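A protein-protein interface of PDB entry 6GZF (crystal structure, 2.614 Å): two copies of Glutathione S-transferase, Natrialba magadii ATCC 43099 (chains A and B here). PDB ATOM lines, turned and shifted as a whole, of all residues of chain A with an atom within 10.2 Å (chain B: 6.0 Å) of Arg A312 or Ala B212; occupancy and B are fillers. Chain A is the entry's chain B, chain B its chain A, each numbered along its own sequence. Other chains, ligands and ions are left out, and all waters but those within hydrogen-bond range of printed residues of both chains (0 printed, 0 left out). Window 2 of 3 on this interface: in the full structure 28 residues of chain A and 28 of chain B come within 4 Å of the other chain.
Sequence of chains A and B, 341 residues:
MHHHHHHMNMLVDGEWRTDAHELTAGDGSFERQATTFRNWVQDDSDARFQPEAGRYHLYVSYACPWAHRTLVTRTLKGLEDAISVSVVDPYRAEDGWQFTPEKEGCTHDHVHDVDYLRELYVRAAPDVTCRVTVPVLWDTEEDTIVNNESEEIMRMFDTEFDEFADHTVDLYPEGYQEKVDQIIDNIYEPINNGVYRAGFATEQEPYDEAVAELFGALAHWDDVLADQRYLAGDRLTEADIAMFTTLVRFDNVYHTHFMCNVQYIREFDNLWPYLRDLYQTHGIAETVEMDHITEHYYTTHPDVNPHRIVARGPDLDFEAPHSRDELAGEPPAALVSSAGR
Hydrophobic or aromatic side chains of chain A within 4 Å of the printed part of chain B: Tyr A264, Tyr A298, Ile A309, Ala A311 and Pro A314. Hydrophobic or aromatic side chains of chain B that line the printed part of chain A: Tyr B207, Val B211, Ala B212, Met B259 and Val B262. Among the printed residues, no Asp or Glu carboxylate lies within 4 Å of a Lys or Arg side-chain nitrogen of the other chain.
OH of Tyr B207 lies within hydrogen-bond range of O of Met B259. The side-chain amide oxygen of Asn B261 sits close to the backbone carbonyl oxygen of Met B259 (3.4 Å). O of Ile A309 is in hydrogen-bond range of ND2 of Asn A305, 2.9 Å away. OH of Tyr A298 sits at hydrogen-bond distance from O of Asn A252 (2.9 Å). ND2 of Asn A305 sits at hydrogen-bond distance from O of Tyr A298, 3.1 Å away.
CG2 of Thr A256 touches CG of Met B259 (3.5 Å). Tyr A264 touches Val B262 (OH to O, 3.9 Å). CE1 of Tyr A298 touches SD of Met B259, at 3.98 Å. Asn B261 touches Tyr A298. Ile A309 touches Met B259 (O to SD, 3.9 Å). Met B259 touches Ala A311. ND2 of Asn B261 touches CB of Ala A311, at 3.7 Å. Arg A312 touches Val B211. OD1 of Asn B261 touches N of Arg A312, at 3.8 Å. Gly A313 touches Val B262.
The backbone carbonyl oxygen of Asn B261 is in hydrogen-bond range of the side-chain hydroxyl of Tyr A264 (3.0 Å). The side-chain hydroxyl (OH) of Tyr B207 lies within hydrogen-bond range of the backbone NH (N) of Arg A312 (3.2 Å). The side-chain amide oxygen (OD1) of Asn B261 lies within hydrogen-bond range of the backbone NH (N) of Gly A313, at 3.0 Å. N of Pro A314 sits close to O of Asn B261 (3.3 Å). The side-chain hydroxyl (OG1) of Thr A256 lies within hydrogen-bond range of the side-chain amide nitrogen (ND2) of Asn B261, at 2.8 Å.
No position is printed for both chains. Of the 22 pairs that touch across the chains among the printed residues, none has its exchanged pair printed and touching as well.
Printed residues of chain B within 4 Å of Tyr A264: Asn B261 and Val B262. Of the printed residues of chain B, Tyr A298 touches Met B259 (3.98 Å) and Asn B261 (3.96 Å). Printed residues of chain B within 4 Å of Arg A312: Tyr B207, Val B211, Ala B212, Asn B261 and Val B262. Leu A316 touches none of the printed residues of chain B. Asp B208 touches none of the printed residues of chain A. Ala B210 touches none of the printed residues of chain A. Val B211 touches just one residue of chain A: Arg A312. Of chain A, only Arg A312 comes within 4 Å of Ala B212. No residue of chain A comes within 4 Å of Gly B216. The nearest printed residue of chain B that does not touch Pro A314 is Phe B215 (8.0 Å).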
ATOM      1  N   ASP A 251     -19.777  20.640  -1.120  1.00  0.00           N
ATOM      2  CA  ASP A 251     -18.634  19.997  -0.479  1.00  0.00           C
ATOM      3  C   ASP A 251     -17.949  18.958  -1.366  1.00  0.00           C
ATOM      4  O   ASP A 251     -16.783  18.630  -1.155  1.00  0.00           O
ATOM      5  CB  ASP A 251     -19.067  19.351   0.838  1.00  0.00           C
ATOM      6  CG  ASP A 251     -19.340  20.374   1.924  1.00  0.00           C
ATOM      7  OD1 ASP A 251     -19.388  21.581   1.604  1.00  0.00           O
ATOM      8  OD2 ASP A 251     -19.504  19.972   3.096  1.00  0.00           O
ATOM      9  N   ASN A 252     -18.670  18.449  -2.359  1.00  0.00           N
ATOM     10  CA  ASN A 252     -18.100  17.463  -3.271  1.00  0.00           C
ATOM     11  C   ASN A 252     -17.536  18.089  -4.544  1.00  0.00           C
ATOM     12  O   ASN A 252     -16.607  17.550  -5.146  1.00  0.00           O
ATOM     13  CB  ASN A 252     -19.142  16.404  -3.637  1.00  0.00           C
ATOM     14  CG  ASN A 252     -19.217  15.280  -2.618  1.00  0.00           C
ATOM     15  OD1 ASN A 252     -18.231  14.968  -1.948  1.00  0.00           O
ATOM     16  ND2 ASN A 252     -20.385  14.661  -2.502  1.00  0.00           N
ATOM     17  N   VAL A 253     -18.095  19.224  -4.955  1.00  0.00           N
ATOM     18  CA  VAL A 253     -17.688  19.852  -6.210  1.00  0.00           C
ATOM     19  C   VAL A 253     -17.300  21.325  -6.061  1.00  0.00           C
ATOM     20  O   VAL A 253     -16.139  21.682  -6.258  1.00  0.00           O
ATOM     21  CB  VAL A 253     -18.802  19.746  -7.274  1.00  0.00           C
ATOM     22  CG1 VAL A 253     -18.407  20.500  -8.534  1.00  0.00           C
ATOM     23  CG2 VAL A 253     -19.099  18.289  -7.595  1.00  0.00           C
ATOM     24  N   THR A 256     -14.085  22.373  -3.996  1.00  0.00           N
ATOM     25  CA  THR A 256     -12.790  22.015  -4.561  1.00  0.00           C
ATOM     26  C   THR A 256     -12.658  22.405  -6.030  1.00  0.00           C
ATOM     27  O   THR A 256     -11.772  23.178  -6.398  1.00  0.00           O
ATOM     28  CB  THR A 256     -12.531  20.506  -4.432  1.00  0.00           C
ATOM     29  OG1 THR A 256     -12.615  20.121  -3.055  1.00  0.00           O
ATOM     30  CG2 THR A 256     -11.154  20.162  -4.965  1.00  0.00           C
ATOM     31  N   HIS A 257     -13.542  21.863  -6.862  1.00  0.00           N
ATOM     32  CA  HIS A 257     -13.476  22.057  -8.307  1.00  0.00           C
ATOM     33  C   HIS A 257     -13.582  23.526  -8.709  1.00  0.00           C
ATOM     34  O   HIS A 257     -12.835  23.994  -9.569  1.00  0.00           O
ATOM     35  CB  HIS A 257     -14.578  21.248  -8.996  1.00  0.00           C
ATOM     36  CG  HIS A 257     -14.554  21.344 -10.489  1.00  0.00           C
ATOM     37  ND1 HIS A 257     -13.474  20.943 -11.244  1.00  0.00           N
ATOM     38  CD2 HIS A 257     -15.482  21.792 -11.368  1.00  0.00           C
ATOM     39  CE1 HIS A 257     -13.735  21.141 -12.524  1.00  0.00           C
ATOM     40  NE2 HIS A 257     -14.948  21.657 -12.626  1.00  0.00           N
ATOM     41  N   TYR A 264     -16.253  24.352   4.423  1.00  0.00           N
ATOM     42  CA  TYR A 264     -17.213  23.299   4.105  1.00  0.00           C
ATOM     43  C   TYR A 264     -18.630  23.714   4.487  1.00  0.00           C
ATOM     44  O   TYR A 264     -18.823  24.499   5.412  1.00  0.00           O
ATOM     45  CB  TYR A 264     -16.857  22.002   4.836  1.00  0.00           C
ATOM     46  CG  TYR A 264     -15.862  21.107   4.131  1.00  0.00           C
ATOM     47  CD1 TYR A 264     -15.822  21.024   2.745  1.00  0.00           C
ATOM     48  CD2 TYR A 264     -14.975  20.328   4.861  1.00  0.00           C
ATOM     49  CE1 TYR A 264     -14.915  20.195   2.107  1.00  0.00           C
ATOM     50  CE2 TYR A 264     -14.068  19.501   4.234  1.00  0.00           C
ATOM     51  CZ  TYR A 264     -14.041  19.436   2.858  1.00  0.00           C
ATOM     52  OH  TYR A 264     -13.136  18.609   2.234  1.00  0.00           O
ATOM     53  N   MET A 290     -25.224  11.607  -7.014  1.00  0.00           N
ATOM     54  CA  MET A 290     -23.913  12.195  -6.764  1.00  0.00           C
ATOM     55  C   MET A 290     -22.879  11.782  -7.807  1.00  0.00           C
ATOM     56  O   MET A 290     -21.976  12.551  -8.130  1.00  0.00           O
ATOM     57  CB  MET A 290     -23.421  11.811  -5.366  1.00  0.00           C
ATOM     58  CG  MET A 290     -22.211  12.598  -4.894  1.00  0.00           C
ATOM     59  SD  MET A 290     -22.554  14.362  -4.751  1.00  0.00           S
ATOM     60  CE  MET A 290     -23.807  14.360  -3.472  1.00  0.00           C
ATOM     61  N   ASP A 291     -23.015  10.570  -8.336  1.00  0.00           N
ATOM     62  CA  ASP A 291     -22.076  10.076  -9.335  1.00  0.00           C
ATOM     63  C   ASP A 291     -22.203  10.871 -10.631  1.00  0.00           C
ATOM     64  O   ASP A 291     -21.202  11.167 -11.283  1.00  0.00           O
ATOM     65  CB  ASP A 291     -22.295   8.587  -9.601  1.00  0.00           C
ATOM     66  CG  ASP A 291     -21.099   7.936 -10.266  1.00  0.00           C
ATOM     67  OD1 ASP A 291     -20.113   7.636  -9.558  1.00  0.00           O
ATOM     68  OD2 ASP A 291     -21.139   7.727 -11.498  1.00  0.00           O
ATOM     69  N   ILE A 293     -23.228  13.930 -10.660  1.00  0.00           N
ATOM     70  CA  ILE A 293     -22.720  15.237 -10.259  1.00  0.00           C
ATOM     71  C   ILE A 293     -21.197  15.295 -10.320  1.00  0.00           C
ATOM     72  O   ILE A 293     -20.629  16.197 -10.936  1.00  0.00           O
ATOM     73  CB  ILE A 293     -23.180  15.598  -8.832  1.00  0.00           C
ATOM     74  CG1 ILE A 293     -24.703  15.727  -8.779  1.00  0.00           C
ATOM     75  CG2 ILE A 293     -22.520  16.887  -8.368  1.00  0.00           C
ATOM     76  CD1 ILE A 293     -25.245  16.019  -7.395  1.00  0.00           C
ATOM     77  N   THR A 294     -20.543  14.328  -9.685  1.00  0.00           N
ATOM     78  CA  THR A 294     -19.086  14.312  -9.614  1.00  0.00           C
ATOM     79  C   THR A 294     -18.442  14.032 -10.968  1.00  0.00           C
ATOM     80  O   THR A 294     -17.375  14.564 -11.272  1.00  0.00           O
ATOM     81  CB  THR A 294     -18.581  13.267  -8.597  1.00  0.00           C
ATOM     82  OG1 THR A 294     -19.040  11.963  -8.976  1.00  0.00           O
ATOM     83  CG2 THR A 294     -19.082  13.597  -7.199  1.00  0.00           C
ATOM     84  N   GLU A 295     -19.084  13.201 -11.784  1.00  0.00           N
ATOM     85  CA  GLU A 295     -18.522  12.866 -13.088  1.00  0.00           C
ATOM     86  C   GLU A 295     -18.546  14.063 -14.030  1.00  0.00           C
ATOM     87  O   GLU A 295     -17.563  14.339 -14.710  1.00  0.00           O
ATOM     88  CB  GLU A 295     -19.268  11.695 -13.731  1.00  0.00           C
ATOM     89  CG  GLU A 295     -18.692  11.293 -15.083  1.00  0.00           C
ATOM     90  CD  GLU A 295     -19.503  10.220 -15.783  1.00  0.00           C
ATOM     91  OE1 GLU A 295     -20.188   9.439 -15.092  1.00  0.00           O
ATOM     92  OE2 GLU A 295     -19.450  10.156 -17.030  1.00  0.00           O
ATOM     93  N   TYR A 298     -16.033  17.250 -13.079  1.00  0.00           N
ATOM     94  CA  TYR A 298     -14.610  16.931 -13.102  1.00  0.00           C
ATOM     95  C   TYR A 298     -14.130  16.403 -14.454  1.00  0.00           C
ATOM     96  O   TYR A 298     -12.930  16.252 -14.666  1.00  0.00           O
ATOM     97  CB  TYR A 298     -14.275  15.912 -12.008  1.00  0.00           C
ATOM     98  CG  TYR A 298     -14.271  16.489 -10.609  1.00  0.00           C
ATOM     99  CD1 TYR A 298     -13.274  17.366 -10.203  1.00  0.00           C
ATOM    100  CD2 TYR A 298     -15.258  16.149  -9.692  1.00  0.00           C
ATOM    101  CE1 TYR A 298     -13.264  17.895  -8.925  1.00  0.00           C
ATOM    102  CE2 TYR A 298     -15.256  16.673  -8.412  1.00  0.00           C
ATOM    103  CZ  TYR A 298     -14.257  17.545  -8.035  1.00  0.00           C
ATOM    104  OH  TYR A 298     -14.251  18.067  -6.761  1.00  0.00           O
ATOM    105  N   ASN A 305     -10.235  21.634 -15.048  1.00  0.00           N
ATOM    106  CA  ASN A 305      -9.595  20.403 -14.603  1.00  0.00           C
ATOM    107  C   ASN A 305      -9.090  19.597 -15.800  1.00  0.00           C
ATOM    108  O   ASN A 305      -9.732  18.632 -16.216  1.00  0.00           O
ATOM    109  CB  ASN A 305     -10.571  19.572 -13.770  1.00  0.00           C
ATOM    110  CG  ASN A 305      -9.901  18.407 -13.072  1.00  0.00           C
ATOM    111  OD1 ASN A 305      -8.712  18.460 -12.755  1.00  0.00           O
ATOM    112  ND2 ASN A 305     -10.663  17.348 -12.826  1.00  0.00           N
ATOM    113  N   ILE A 309      -9.582  14.405 -13.752  1.00  0.00           N
ATOM    114  CA  ILE A 309      -9.600  13.472 -12.630  1.00  0.00           C
ATOM    115  C   ILE A 309     -10.714  13.826 -11.650  1.00  0.00           C
ATOM    116  O   ILE A 309     -10.816  14.967 -11.199  1.00  0.00           O
ATOM    117  CB  ILE A 309      -8.252  13.458 -11.881  1.00  0.00           C
ATOM    118  CG1 ILE A 309      -7.128  13.012 -12.817  1.00  0.00           C
ATOM    119  CG2 ILE A 309      -8.328  12.546 -10.665  1.00  0.00           C
ATOM    120  CD1 ILE A 309      -7.355  11.646 -13.429  1.00  0.00           C
ATOM    121  N   VAL A 310     -11.551  12.844 -11.328  1.00  0.00           N
ATOM    122  CA  VAL A 310     -12.643  13.051 -10.384  1.00  0.00           C
ATOM    123  C   VAL A 310     -12.144  12.988  -8.945  1.00  0.00           C
ATOM    124  O   VAL A 310     -11.619  11.966  -8.504  1.00  0.00           O
ATOM    125  CB  VAL A 310     -13.762  12.010 -10.577  1.00  0.00           C
ATOM    126  CG1 VAL A 310     -14.814  12.152  -9.487  1.00  0.00           C
ATOM    127  CG2 VAL A 310     -14.388  12.152 -11.957  1.00  0.00           C
ATOM    128  N   ALA A 311     -12.308  14.088  -8.218  1.00  0.00           N
ATOM    129  CA  ALA A 311     -11.883  14.155  -6.826  1.00  0.00           C
ATOM    130  C   ALA A 311     -12.715  13.217  -5.962  1.00  0.00           C
ATOM    131  O   ALA A 311     -13.860  12.905  -6.291  1.00  0.00           O
ATOM    132  CB  ALA A 311     -11.978  15.582  -6.308  1.00  0.00           C
ATOM    133  N   ARG A 312     -12.133  12.767  -4.855  1.00  0.00           N
ATOM    134  CA  ARG A 312     -12.805  11.830  -3.964  1.00  0.00           C
ATOM    135  C   ARG A 312     -13.881  12.517  -3.127  1.00  0.00           C
ATOM    136  O   ARG A 312     -15.006  12.027  -3.026  1.00  0.00           O
ATOM    137  CB  ARG A 312     -11.784  11.142  -3.056  1.00  0.00           C
ATOM    138  CG  ARG A 312     -12.392  10.256  -1.981  1.00  0.00           C
ATOM    139  CD  ARG A 312     -11.452   9.116  -1.628  1.00  0.00           C
ATOM    140  NE  ARG A 312     -11.710   8.575  -0.298  1.00  0.00           N
ATOM    141  CZ  ARG A 312     -11.067   7.535   0.222  1.00  0.00           C
ATOM    142  NH1 ARG A 312     -10.129   6.915  -0.483  1.00  0.00           N
ATOM    143  NH2 ARG A 312     -11.363   7.109   1.442  1.00  0.00           N
ATOM    144  N   GLY A 313     -13.530  13.650  -2.529  1.00  0.00           N
ATOM    145  CA  GLY A 313     -14.466  14.396  -1.709  1.00  0.00           C
ATOM    146  C   GLY A 313     -14.644  13.791  -0.330  1.00  0.00           C
ATOM    147  O   GLY A 313     -14.213  12.665  -0.082  1.00  0.00           O
ATOM    148  N   PRO A 314     -15.284  14.540   0.578  1.00  0.00           N
ATOM    149  CA  PRO A 314     -15.500  14.093   1.958  1.00  0.00           C
ATOM    150  C   PRO A 314     -16.498  12.946   2.062  1.00  0.00           C
ATOM    151  O   PRO A 314     -17.262  12.703   1.127  1.00  0.00           O
ATOM    152  CB  PRO A 314     -16.044  15.347   2.650  1.00  0.00           C
ATOM    153  CG  PRO A 314     -16.675  16.133   1.556  1.00  0.00           C
ATOM    154  CD  PRO A 314     -15.825  15.890   0.344  1.00  0.00           C
ATOM    155  N   ASP A 315     -16.484  12.249   3.192  1.00  0.00           N
ATOM    156  CA  ASP A 315     -17.443  11.183   3.448  1.00  0.00           C
ATOM    157  C   ASP A 315     -18.675  11.754   4.142  1.00  0.00           C
ATOM    158  O   ASP A 315     -18.800  11.689   5.365  1.00  0.00           O
ATOM    159  CB  ASP A 315     -16.812  10.078   4.296  1.00  0.00           C
ATOM    160  CG  ASP A 315     -17.750   8.908   4.526  1.00  0.00           C
ATOM    161  OD1 ASP A 315     -17.998   8.148   3.566  1.00  0.00           O
ATOM    162  OD2 ASP A 315     -18.237   8.748   5.665  1.00  0.00           O
ATOM    163  N   LEU A 316     -19.579  12.320   3.348  1.00  0.00           N
ATOM    164  CA  LEU A 316     -20.769  12.977   3.874  1.00  0.00           C
ATOM    165  C   LEU A 316     -21.880  11.986   4.192  1.00  0.00           C
ATOM    166  O   LEU A 316     -22.287  11.201   3.335  1.00  0.00           O
ATOM    167  CB  LEU A 316     -21.281  14.020   2.880  1.00  0.00           C
ATOM    168  CG  LEU A 316     -20.361  15.203   2.576  1.00  0.00           C
ATOM    169  CD1 LEU A 316     -20.667  15.774   1.200  1.00  0.00           C
ATOM    170  CD2 LEU A 316     -20.503  16.273   3.644  1.00  0.00           C
ATOM    171  N   TYR B 207      -4.471   8.354  -8.632  1.00  0.00           N
ATOM    172  CA  TYR B 207      -5.021   9.376  -7.747  1.00  0.00           C
ATOM    173  C   TYR B 207      -5.746   8.745  -6.564  1.00  0.00           C
ATOM    174  O   TYR B 207      -5.570   9.166  -5.421  1.00  0.00           O
ATOM    175  CB  TYR B 207      -5.973  10.300  -8.513  1.00  0.00           C
ATOM    176  CG  TYR B 207      -6.804  11.207  -7.627  1.00  0.00           C
ATOM    177  CD1 TYR B 207      -6.318  12.440  -7.214  1.00  0.00           C
ATOM    178  CD2 TYR B 207      -8.078  10.833  -7.214  1.00  0.00           C
ATOM    179  CE1 TYR B 207      -7.073  13.272  -6.406  1.00  0.00           C
ATOM    180  CE2 TYR B 207      -8.838  11.657  -6.406  1.00  0.00           C
ATOM    181  CZ  TYR B 207      -8.332  12.875  -6.008  1.00  0.00           C
ATOM    182  OH  TYR B 207      -9.089  13.696  -5.204  1.00  0.00           O
ATOM    183  N   ASP B 208      -6.566   7.739  -6.854  1.00  0.00           N
ATOM    184  CA  ASP B 208      -7.358   7.062  -5.831  1.00  0.00           C
ATOM    185  C   ASP B 208      -6.481   6.479  -4.727  1.00  0.00           C
ATOM    186  O   ASP B 208      -6.782   6.629  -3.544  1.00  0.00           O
ATOM    187  CB  ASP B 208      -8.206   5.954  -6.463  1.00  0.00           C
ATOM    188  CG  ASP B 208      -9.258   6.495  -7.412  1.00  0.00           C
ATOM    189  OD1 ASP B 208      -9.663   7.665  -7.247  1.00  0.00           O
ATOM    190  OD2 ASP B 208      -9.679   5.751  -8.323  1.00  0.00           O
ATOM    191  N   GLU B 209      -5.397   5.819  -5.120  1.00  0.00           N
ATOM    192  CA  GLU B 209      -4.465   5.237  -4.161  1.00  0.00           C
ATOM    193  C   GLU B 209      -3.741   6.316  -3.363  1.00  0.00           C
ATOM    194  O   GLU B 209      -3.573   6.195  -2.150  1.00  0.00           O
ATOM    195  CB  GLU B 209      -3.445   4.349  -4.874  1.00  0.00           C
ATOM    196  CG  GLU B 209      -4.027   3.081  -5.470  1.00  0.00           C
ATOM    197  CD  GLU B 209      -3.014   2.313  -6.296  1.00  0.00           C
ATOM    198  OE1 GLU B 209      -1.804   2.416  -5.999  1.00  0.00           O
ATOM    199  OE2 GLU B 209      -3.423   1.607  -7.242  1.00  0.00           O
ATOM    200  N   ALA B 210      -3.316   7.369  -4.056  1.00  0.00           N
ATOM    201  CA  ALA B 210      -2.581   8.461  -3.429  1.00  0.00           C
ATOM    202  C   ALA B 210      -3.425   9.166  -2.374  1.00  0.00           C
ATOM    203  O   ALA B 210      -2.911   9.591  -1.341  1.00  0.00           O
ATOM    204  CB  ALA B 210      -2.112   9.454  -4.481  1.00  0.00           C
ATOM    205  N   VAL B 211      -4.722   9.282  -2.635  1.00  0.00           N
ATOM    206  CA  VAL B 211      -5.641   9.918  -1.698  1.00  0.00           C
ATOM    207  C   VAL B 211      -5.996   8.975  -0.550  1.00  0.00           C
ATOM    208  O   VAL B 211      -6.019   9.382   0.614  1.00  0.00           O
ATOM    209  CB  VAL B 211      -6.931  10.378  -2.405  1.00  0.00           C
ATOM    210  CG1 VAL B 211      -7.960  10.854  -1.391  1.00  0.00           C
ATOM    211  CG2 VAL B 211      -6.619  11.477  -3.402  1.00  0.00           C
ATOM    212  N   ALA B 212      -6.262   7.716  -0.884  1.00  0.00           N
ATOM    213  CA  ALA B 212      -6.615   6.711   0.113  1.00  0.00           C
ATOM    214  C   ALA B 212      -5.491   6.512   1.125  1.00  0.00           C
ATOM    215  O   ALA B 212      -5.728   6.500   2.332  1.00  0.00           O
ATOM    216  CB  ALA B 212      -6.956   5.392  -0.562  1.00  0.00           C
ATOM    217  N   GLU B 213      -4.268   6.365   0.624  1.00  0.00           N
ATOM    218  CA  GLU B 213      -3.103   6.175   1.482  1.00  0.00           C
ATOM    219  C   GLU B 213      -2.816   7.411   2.327  1.00  0.00           C
ATOM    220  O   GLU B 213      -2.418   7.301   3.486  1.00  0.00           O
ATOM    221  CB  GLU B 213      -1.874   5.825   0.640  1.00  0.00           C
ATOM    222  CG  GLU B 213      -1.809   4.372   0.202  1.00  0.00           C
ATOM    223  CD  GLU B 213      -0.675   3.617   0.868  1.00  0.00           C
ATOM    224  OE1 GLU B 213       0.219   4.271   1.447  1.00  0.00           O
ATOM    225  OE2 GLU B 213      -0.676   2.368   0.814  1.00  0.00           O
ATOM    226  N   LEU B 214      -3.023   8.585   1.737  1.00  0.00           N
ATOM    227  CA  LEU B 214      -2.745   9.853   2.404  1.00  0.00           C
ATOM    228  C   LEU B 214      -3.595  10.052   3.654  1.00  0.00           C
ATOM    229  O   LEU B 214      -3.067  10.198   4.756  1.00  0.00           O
ATOM    230  CB  LEU B 214      -2.968  11.017   1.436  1.00  0.00           C
ATOM    231  CG  LEU B 214      -2.985  12.443   1.994  1.00  0.00           C
ATOM    232  CD1 LEU B 214      -1.691  12.771   2.726  1.00  0.00           C
ATOM    233  CD2 LEU B 214      -3.234  13.437   0.872  1.00  0.00           C
ATOM    234  N   PHE B 215      -4.913  10.064   3.478  1.00  0.00           N
ATOM    235  CA  PHE B 215      -5.824  10.311   4.589  1.00  0.00           C
ATOM    236  C   PHE B 215      -5.877   9.125   5.545  1.00  0.00           C
ATOM    237  O   PHE B 215      -6.294   9.263   6.695  1.00  0.00           O
ATOM    238  CB  PHE B 215      -7.221  10.640   4.062  1.00  0.00           C
ATOM    239  CG  PHE B 215      -7.340  12.033   3.516  1.00  0.00           C
ATOM    240  CD1 PHE B 215      -7.673  13.090   4.347  1.00  0.00           C
ATOM    241  CD2 PHE B 215      -7.100  12.289   2.176  1.00  0.00           C
ATOM    242  CE1 PHE B 215      -7.776  14.376   3.850  1.00  0.00           C
ATOM    243  CE2 PHE B 215      -7.200  13.573   1.673  1.00  0.00           C
ATOM    244  CZ  PHE B 215      -7.539  14.618   2.512  1.00  0.00           C
ATOM    245  N   GLY B 216      -5.450   7.963   5.065  1.00  0.00           N
ATOM    246  CA  GLY B 216      -5.288   6.809   5.927  1.00  0.00           C
ATOM    247  C   GLY B 216      -4.119   7.044   6.861  1.00  0.00           C
ATOM    248  O   GLY B 216      -4.199   6.772   8.059  1.00  0.00           O
ATOM    249  N   ALA B 217      -3.029   7.564   6.303  1.00  0.00           N
ATOM    250  CA  ALA B 217      -1.836   7.882   7.079  1.00  0.00           C
ATOM    251  C   ALA B 217      -2.104   9.009   8.071  1.00  0.00           C
ATOM    252  O   ALA B 217      -1.632   8.974   9.207  1.00  0.00           O
ATOM    253  CB  ALA B 217      -0.687   8.253   6.155  1.00  0.00           C
ATOM    254  N   MET B 259      -6.438  18.704  -5.009  1.00  0.00           N
ATOM    255  CA  MET B 259      -7.667  17.924  -4.878  1.00  0.00           C
ATOM    256  C   MET B 259      -7.588  16.818  -3.825  1.00  0.00           C
ATOM    257  O   MET B 259      -8.191  15.757  -3.985  1.00  0.00           O
ATOM    258  CB  MET B 259      -8.055  17.323  -6.232  1.00  0.00           C
ATOM    259  CG  MET B 259      -9.086  18.141  -6.993  1.00  0.00           C
ATOM    260  SD  MET B 259      -9.303  17.625  -8.705  1.00  0.00           S
ATOM    261  CE  MET B 259      -8.057  18.624  -9.514  1.00  0.00           C
ATOM    262  N   ASN B 261      -9.194  16.401  -1.063  1.00  0.00           N
ATOM    263  CA  ASN B 261     -10.331  17.033  -0.401  1.00  0.00           C
ATOM    264  C   ASN B 261     -11.239  16.100   0.398  1.00  0.00           C
ATOM    265  O   ASN B 261     -12.458  16.275   0.402  1.00  0.00           O
ATOM    266  CB  ASN B 261     -11.173  17.769  -1.446  1.00  0.00           C
ATOM    267  CG  ASN B 261     -11.791  16.828  -2.465  1.00  0.00           C
ATOM    268  OD1 ASN B 261     -11.334  15.699  -2.644  1.00  0.00           O
ATOM    269  ND2 ASN B 261     -12.840  17.292  -3.138  1.00  0.00           N
ATOM    270  N   VAL B 262     -10.659  15.121   1.080  1.00  0.00           N
ATOM    271  CA  VAL B 262     -11.450  14.252   1.942  1.00  0.00           C
ATOM    272  C   VAL B 262     -11.803  14.978   3.237  1.00  0.00           C
ATOM    273  O   VAL B 262     -12.948  14.944   3.687  1.00  0.00           O
ATOM    274  CB  VAL B 262     -10.714  12.939   2.269  1.00  0.00           C
ATOM    275  CG1 VAL B 262     -11.506  12.121   3.279  1.00  0.00           C
ATOM    276  CG2 VAL B 262     -10.476  12.137   0.998  1.00  0.00           C
